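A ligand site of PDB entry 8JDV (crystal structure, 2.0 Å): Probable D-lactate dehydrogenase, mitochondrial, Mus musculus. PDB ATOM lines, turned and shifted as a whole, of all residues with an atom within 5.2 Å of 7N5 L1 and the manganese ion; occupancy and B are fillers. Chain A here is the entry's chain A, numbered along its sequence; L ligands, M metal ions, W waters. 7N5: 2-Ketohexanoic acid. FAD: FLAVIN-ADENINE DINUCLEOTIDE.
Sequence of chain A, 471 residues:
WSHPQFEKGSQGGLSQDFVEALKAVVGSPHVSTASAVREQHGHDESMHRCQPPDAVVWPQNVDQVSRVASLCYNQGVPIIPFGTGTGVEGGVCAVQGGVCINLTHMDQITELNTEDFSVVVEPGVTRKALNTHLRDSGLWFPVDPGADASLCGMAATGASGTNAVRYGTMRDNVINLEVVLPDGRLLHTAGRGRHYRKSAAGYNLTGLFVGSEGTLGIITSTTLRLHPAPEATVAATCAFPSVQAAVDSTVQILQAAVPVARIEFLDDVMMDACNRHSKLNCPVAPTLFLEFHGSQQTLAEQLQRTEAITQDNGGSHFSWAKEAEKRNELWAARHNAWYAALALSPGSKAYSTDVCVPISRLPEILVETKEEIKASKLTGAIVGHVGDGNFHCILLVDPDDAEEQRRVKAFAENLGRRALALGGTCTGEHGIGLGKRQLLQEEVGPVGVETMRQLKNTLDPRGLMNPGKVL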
ATOM      1  N   VAL A  88     -30.465  22.051  27.099  1.00  0.00           N
ATOM      2  CA  VAL A  88     -30.802  22.468  25.749  1.00  0.00           C
ATOM      3  C   VAL A  88     -32.240  22.111  25.381  1.00  0.00           C
ATOM      4  O   VAL A  88     -32.586  22.076  24.200  1.00  0.00           O
ATOM      5  CB  VAL A  88     -29.820  21.893  24.726  1.00  0.00           C
ATOM      6  CG1 VAL A  88     -28.412  22.368  25.071  1.00  0.00           C
ATOM      7  CG2 VAL A  88     -29.886  20.367  24.694  1.00  0.00           C
ATOM      8  N   ARG A 334     -13.794  19.369  20.158  1.00  0.00           N
ATOM      9  CA  ARG A 334     -15.028  18.591  20.125  1.00  0.00           C
ATOM     10  C   ARG A 334     -16.037  19.116  21.143  1.00  0.00           C
ATOM     11  O   ARG A 334     -17.204  19.364  20.810  1.00  0.00           O
ATOM     12  CB  ARG A 334     -14.742  17.110  20.356  1.00  0.00           C
ATOM     13  CG  ARG A 334     -15.998  16.277  20.635  1.00  0.00           C
ATOM     14  CD  ARG A 334     -16.971  16.287  19.455  1.00  0.00           C
ATOM     15  NE  ARG A 334     -18.189  15.545  19.797  1.00  0.00           N
ATOM     16  CZ  ARG A 334     -19.282  16.071  20.347  1.00  0.00           C
ATOM     17  NH1 ARG A 334     -19.339  17.374  20.633  1.00  0.00           N
ATOM     18  NH2 ARG A 334     -20.314  15.283  20.631  1.00  0.00           N
ATOM     19  N   HIS A 335     -15.603  19.292  22.394  1.00  0.00           N
ATOM     20  CA  HIS A 335     -16.525  19.713  23.458  1.00  0.00           C
ATOM     21  C   HIS A 335     -17.145  21.067  23.166  1.00  0.00           C
ATOM     22  O   HIS A 335     -18.225  21.388  23.698  1.00  0.00           O
ATOM     23  CB  HIS A 335     -15.799  19.747  24.799  1.00  0.00           C
ATOM     24  CG  HIS A 335     -15.636  18.397  25.435  1.00  0.00           C
ATOM     25  ND1 HIS A 335     -14.507  18.037  26.138  1.00  0.00           N
ATOM     26  CD2 HIS A 335     -16.444  17.310  25.447  1.00  0.00           C
ATOM     27  CE1 HIS A 335     -14.630  16.791  26.574  1.00  0.00           C
ATOM     28  NE2 HIS A 335     -15.798  16.321  26.158  1.00  0.00           N
ATOM     29  N   ALA A 337     -18.096  22.047  20.113  1.00  0.00           N
ATOM     30  CA  ALA A 337     -18.710  21.996  18.788  1.00  0.00           C
ATOM     31  C   ALA A 337     -19.973  22.855  18.714  1.00  0.00           C
ATOM     32  O   ALA A 337     -20.251  23.468  17.676  1.00  0.00           O
ATOM     33  CB  ALA A 337     -19.035  20.557  18.408  1.00  0.00           C
ATOM     34  N   TRP A 338     -20.773  22.879  19.786  1.00  0.00           N
ATOM     35  CA  TRP A 338     -21.955  23.733  19.815  1.00  0.00           C
ATOM     36  C   TRP A 338     -21.595  25.185  19.535  1.00  0.00           C
ATOM     37  O   TRP A 338     -22.206  25.843  18.692  1.00  0.00           O
ATOM     38  CB  TRP A 338     -22.624  23.592  21.186  1.00  0.00           C
ATOM     39  CG  TRP A 338     -23.787  24.469  21.519  1.00  0.00           C
ATOM     40  CD1 TRP A 338     -23.803  25.499  22.422  1.00  0.00           C
ATOM     41  CD2 TRP A 338     -25.124  24.345  21.036  1.00  0.00           C
ATOM     42  NE1 TRP A 338     -25.066  26.024  22.513  1.00  0.00           N
ATOM     43  CE2 TRP A 338     -25.896  25.336  21.684  1.00  0.00           C
ATOM     44  CE3 TRP A 338     -25.759  23.485  20.120  1.00  0.00           C
ATOM     45  CZ2 TRP A 338     -27.259  25.504  21.419  1.00  0.00           C
ATOM     46  CZ3 TRP A 338     -27.105  23.652  19.873  1.00  0.00           C
ATOM     47  CH2 TRP A 338     -27.850  24.648  20.529  1.00  0.00           C
ATOM     48  N   SER A 352     -30.808  21.504  18.705  1.00  0.00           N
ATOM     49  CA  SER A 352     -30.043  20.284  18.540  1.00  0.00           C
ATOM     50  C   SER A 352     -30.992  19.110  18.595  1.00  0.00           C
ATOM     51  O   SER A 352     -31.856  19.034  19.479  1.00  0.00           O
ATOM     52  CB  SER A 352     -28.963  20.143  19.602  1.00  0.00           C
ATOM     53  OG  SER A 352     -28.175  18.992  19.327  1.00  0.00           O
ATOM     54  N   VAL A 383     -22.735  16.105  14.493  1.00  0.00           N
ATOM     55  CA  VAL A 383     -21.677  15.680  15.383  1.00  0.00           C
ATOM     56  C   VAL A 383     -22.272  14.670  16.361  1.00  0.00           C
ATOM     57  O   VAL A 383     -23.454  14.759  16.706  1.00  0.00           O
ATOM     58  CB  VAL A 383     -21.045  16.903  16.103  1.00  0.00           C
ATOM     59  CG1 VAL A 383     -22.052  17.561  17.086  1.00  0.00           C
ATOM     60  CG2 VAL A 383     -19.779  16.494  16.829  1.00  0.00           C
ATOM     61  N   HIS A 385     -22.006  11.073  19.344  1.00  0.00           N
ATOM     62  CA  HIS A 385     -21.584   9.873  20.054  1.00  0.00           C
ATOM     63  C   HIS A 385     -22.085   8.657  19.296  1.00  0.00           C
ATOM     64  O   HIS A 385     -22.945   7.897  19.756  1.00  0.00           O
ATOM     65  CB  HIS A 385     -22.156   9.895  21.475  1.00  0.00           C
ATOM     66  CG  HIS A 385     -22.081  11.238  22.149  1.00  0.00           C
ATOM     67  ND1 HIS A 385     -20.885  11.898  22.346  1.00  0.00           N
ATOM     68  CD2 HIS A 385     -23.040  12.045  22.639  1.00  0.00           C
ATOM     69  CE1 HIS A 385     -21.113  13.045  22.946  1.00  0.00           C
ATOM     70  NE2 HIS A 385     -22.418  13.169  23.139  1.00  0.00           N
ATOM     71  N   ASN A 390     -26.020   7.327  18.669  1.00  0.00           N
ATOM     72  CA  ASN A 390     -26.528   8.673  18.926  1.00  0.00           C
ATOM     73  C   ASN A 390     -25.774   9.739  18.127  1.00  0.00           C
ATOM     74  O   ASN A 390     -24.602   9.561  17.793  1.00  0.00           O
ATOM     75  CB  ASN A 390     -26.522   8.804  20.483  1.00  0.00           C
ATOM     76  CG  ASN A 390     -26.778  10.195  21.032  1.00  0.00           C
ATOM     77  OD1 ASN A 390     -25.901  10.756  21.694  1.00  0.00           O
ATOM     78  ND2 ASN A 390     -27.945  10.758  20.755  1.00  0.00           N
ATOM     79  N   HIS A 392     -26.069  14.334  17.022  1.00  0.00           N
ATOM     80  CA  HIS A 392     -26.763  15.612  17.096  1.00  0.00           C
ATOM     81  C   HIS A 392     -26.727  16.246  15.727  1.00  0.00           C
ATOM     82  O   HIS A 392     -25.693  16.255  15.056  1.00  0.00           O
ATOM     83  CB  HIS A 392     -26.091  16.551  18.112  1.00  0.00           C
ATOM     84  CG  HIS A 392     -25.799  15.898  19.431  1.00  0.00           C
ATOM     85  ND1 HIS A 392     -26.791  15.366  20.223  1.00  0.00           N
ATOM     86  CD2 HIS A 392     -24.631  15.677  20.075  1.00  0.00           C
ATOM     87  CE1 HIS A 392     -26.238  14.848  21.309  1.00  0.00           C
ATOM     88  NE2 HIS A 392     -24.932  15.028  21.246  1.00  0.00           N
ATOM     89  N   GLU A 429     -29.641  11.577  25.332  1.00  0.00           N
ATOM     90  CA  GLU A 429     -29.000  12.130  26.526  1.00  0.00           C
ATOM     91  C   GLU A 429     -29.507  13.516  26.966  1.00  0.00           C
ATOM     92  O   GLU A 429     -29.432  13.822  28.160  1.00  0.00           O
ATOM     93  CB  GLU A 429     -27.474  12.170  26.301  1.00  0.00           C
ATOM     94  CG  GLU A 429     -27.136  13.112  25.155  1.00  0.00           C
ATOM     95  CD  GLU A 429     -25.648  13.356  24.909  1.00  0.00           C
ATOM     96  OE1 GLU A 429     -24.745  12.878  25.658  1.00  0.00           O
ATOM     97  OE2 GLU A 429     -25.384  14.171  24.019  1.00  0.00           O
ATOM     98  N   HIS A 430     -30.002  14.372  26.047  1.00  0.00           N
ATOM     99  CA  HIS A 430     -30.368  15.733  26.439  1.00  0.00           C
ATOM    100  C   HIS A 430     -31.658  15.803  27.251  1.00  0.00           C
ATOM    101  O   HIS A 430     -31.832  16.729  28.046  1.00  0.00           O
ATOM    102  CB  HIS A 430     -30.546  16.644  25.204  1.00  0.00           C
ATOM    103  CG  HIS A 430     -29.279  16.910  24.460  1.00  0.00           C
ATOM    104  ND1 HIS A 430     -29.255  17.247  23.134  1.00  0.00           N
ATOM    105  CD2 HIS A 430     -27.979  16.857  24.856  1.00  0.00           C
ATOM    106  CE1 HIS A 430     -27.999  17.411  22.740  1.00  0.00           C
ATOM    107  NE2 HIS A 430     -27.213  17.180  23.760  1.00  0.00           N
HETATM  108  C3  7N5 L   1     -24.055  19.514  22.474  1.00  0.00           C
HETATM  109  C5  7N5 L   1     -26.041  21.027  22.332  1.00  0.00           C
HETATM  110  C4  7N5 L   1     -25.549  19.646  22.687  1.00  0.00           C
HETATM  111  C2  7N5 L   1     -23.698  18.058  22.728  1.00  0.00           C
HETATM  112  C6  7N5 L   1     -25.353  22.001  23.276  1.00  0.00           C
HETATM  113  C1  7N5 L   1     -22.330  17.594  22.249  1.00  0.00           C
HETATM  114  O1A 7N5 L   1     -22.026  16.375  22.207  1.00  0.00           O
HETATM  115  O1B 7N5 L   1     -21.482  18.473  21.876  1.00  0.00           O
HETATM  116  O2  7N5 L   1     -24.458  17.313  23.268  1.00  0.00           O
HETATM  117  PA  FAD L   2     -29.979  22.995  33.904  1.00  0.00           P
HETATM  118  O1A FAD L   2     -29.679  23.897  35.044  1.00  0.00           O
HETATM  119  O2A FAD L   2     -30.198  23.603  32.521  1.00  0.00           O
HETATM  120  O5B FAD L   2     -31.209  22.076  34.198  1.00  0.00           O
HETATM  121  C5B FAD L   2     -31.634  21.066  33.250  1.00  0.00           C
HETATM  122  C4B FAD L   2     -32.883  20.353  33.723  1.00  0.00           C
HETATM  123  O4B FAD L   2     -32.577  19.580  34.902  1.00  0.00           O
HETATM  124  C3B FAD L   2     -34.044  21.264  34.125  1.00  0.00           C
HETATM  125  O3B FAD L   2     -35.293  20.623  33.918  1.00  0.00           O
HETATM  126  C2B FAD L   2     -33.794  21.488  35.618  1.00  0.00           C
HETATM  127  O2B FAD L   2     -34.992  21.847  36.309  1.00  0.00           O
HETATM  128  C1B FAD L   2     -33.259  20.128  36.041  1.00  0.00           C
HETATM  129  N9A FAD L   2     -32.315  20.145  37.153  1.00  0.00           N
HETATM  130  C8A FAD L   2     -31.082  20.732  37.207  1.00  0.00           C
HETATM  131  N7A FAD L   2     -30.444  20.541  38.335  1.00  0.00           N
HETATM  132  C5A FAD L   2     -31.310  19.749  39.069  1.00  0.00           C
HETATM  133  C6A FAD L   2     -31.222  19.163  40.352  1.00  0.00           C
HETATM  134  N6A FAD L   2     -30.171  19.317  41.171  1.00  0.00           N
HETATM  135  N1A FAD L   2     -32.273  18.435  40.778  1.00  0.00           N
HETATM  136  C2A FAD L   2     -33.324  18.272  39.965  1.00  0.00           C
HETATM  137  N3A FAD L   2     -33.519  18.757  38.741  1.00  0.00           N
HETATM  138  C4A FAD L   2     -32.465  19.486  38.352  1.00  0.00           C
HETATM  139  N1  FAD L   2     -25.617  17.106  27.600  1.00  0.00           N
HETATM  140  C2  FAD L   2     -25.311  15.779  27.470  1.00  0.00           C
HETATM  141  O2  FAD L   2     -25.999  14.892  27.983  1.00  0.00           O
HETATM  142  N3  FAD L   2     -24.187  15.397  26.742  1.00  0.00           N
HETATM  143  C4  FAD L   2     -23.316  16.232  26.109  1.00  0.00           C
HETATM  144  O4  FAD L   2     -22.371  15.753  25.478  1.00  0.00           O
HETATM  145  C4X FAD L   2     -23.636  17.636  26.263  1.00  0.00           C
HETATM  146  N5  FAD L   2     -22.828  18.531  25.678  1.00  0.00           N
HETATM  147  C5X FAD L   2     -23.144  19.873  25.831  1.00  0.00           C
HETATM  148  C6  FAD L   2     -22.310  20.827  25.245  1.00  0.00           C
HETATM  149  C7  FAD L   2     -22.579  22.190  25.359  1.00  0.00           C
HETATM  150  C7M FAD L   2     -21.670  23.197  24.696  1.00  0.00           C
HETATM  151  C8  FAD L   2     -23.712  22.611  26.091  1.00  0.00           C
HETATM  152  C8M FAD L   2     -24.044  24.075  26.226  1.00  0.00           C
HETATM  153  C9  FAD L   2     -24.546  21.666  26.671  1.00  0.00           C
HETATM  154  C9A FAD L   2     -24.267  20.300  26.554  1.00  0.00           C
HETATM  155  N10 FAD L   2     -25.085  19.330  27.168  1.00  0.00           N
HETATM  156  C10 FAD L   2     -24.801  17.981  27.024  1.00  0.00           C
HETATM  157  C1' FAD L   2     -26.333  19.713  27.857  1.00  0.00           C
HETATM  158  C2' FAD L   2     -26.189  20.005  29.338  1.00  0.00           C
HETATM  159  O2' FAD L   2     -24.857  20.397  29.662  1.00  0.00           O
HETATM  160  C3' FAD L   2     -26.621  18.765  30.126  1.00  0.00           C
HETATM  161  O3' FAD L   2     -27.991  18.484  29.856  1.00  0.00           O
HETATM  162  C4' FAD L   2     -26.465  18.960  31.624  1.00  0.00           C
HETATM  163  O4' FAD L   2     -26.794  17.737  32.263  1.00  0.00           O
HETATM  164  C5' FAD L   2     -27.343  20.084  32.124  1.00  0.00           C
HETATM  165  O5' FAD L   2     -26.998  20.370  33.498  1.00  0.00           O
HETATM  166  P   FAD L   2     -27.328  21.772  34.133  1.00  0.00           P
HETATM  167  O1P FAD L   2     -27.138  21.749  35.649  1.00  0.00           O
HETATM  168  O2P FAD L   2     -26.572  22.855  33.414  1.00  0.00           O
HETATM  169  O3P FAD L   2     -28.876  21.865  33.783  1.00  0.00           O
HETATM  170 MN    MN M   1     -23.677  15.138  23.245  1.00  0.00          MN
HETATM  171  O   HOH W   1     -19.609  17.502  24.162  1.00  0.00           O
HETATM  172  O   HOH W   2     -20.507  20.897  21.924  1.00  0.00           O
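The manganese ion is bound by OE2 of Glu 429 (2.1 Å), O1A of 7N5 L1 (2.3 Å), O2 of 7N5 L1 (2.3 Å), NE2 of His 385 (2.3 Å), NE2 of His 392 (2.4 Å) and O4 of FAD L2 (2.7 Å).
The manganese ion has six donor atoms within binding distance.
The backbone carbonyl oxygen (O) of His 385 sits at hydrogen-bond distance from the backbone NH (N) of Asn 390 (3.3 Å).
The backbone carbonyl oxygen (O) of Val 383 lies within hydrogen-bond range of the backbone NH (N) of His 392 (2.7 Å).
Val 88 touches 7N5 L1 (CG1 to C6, 3.6 Å).
CD2 of Trp 338 touches C6 of 7N5 L1, 3.3 Å away.
Seven residues have an atom within 4 Å of 7N5 L1: Val 88, Arg 334, Trp 338, His 385, His 392, Glu 429 and His 430.
Water W2 lies within hydrogen-bond range of O1B of 7N5 L1, N of Trp 338, O of His 335 and N of Ala 337.
An oxygen (O1B) of 7N5 L1 lies within salt-bridge range of the guanidinium group of Arg 334, 2.7 Å away.
NE2 of His 430 sits close to O2 of 7N5 L1, at 2.8 Å.
Of the 12 residues printed, 3 come within 4 Å of the manganese ion.
Along chain A the residues within 4 Å of the manganese ion span positions 385 to 429.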
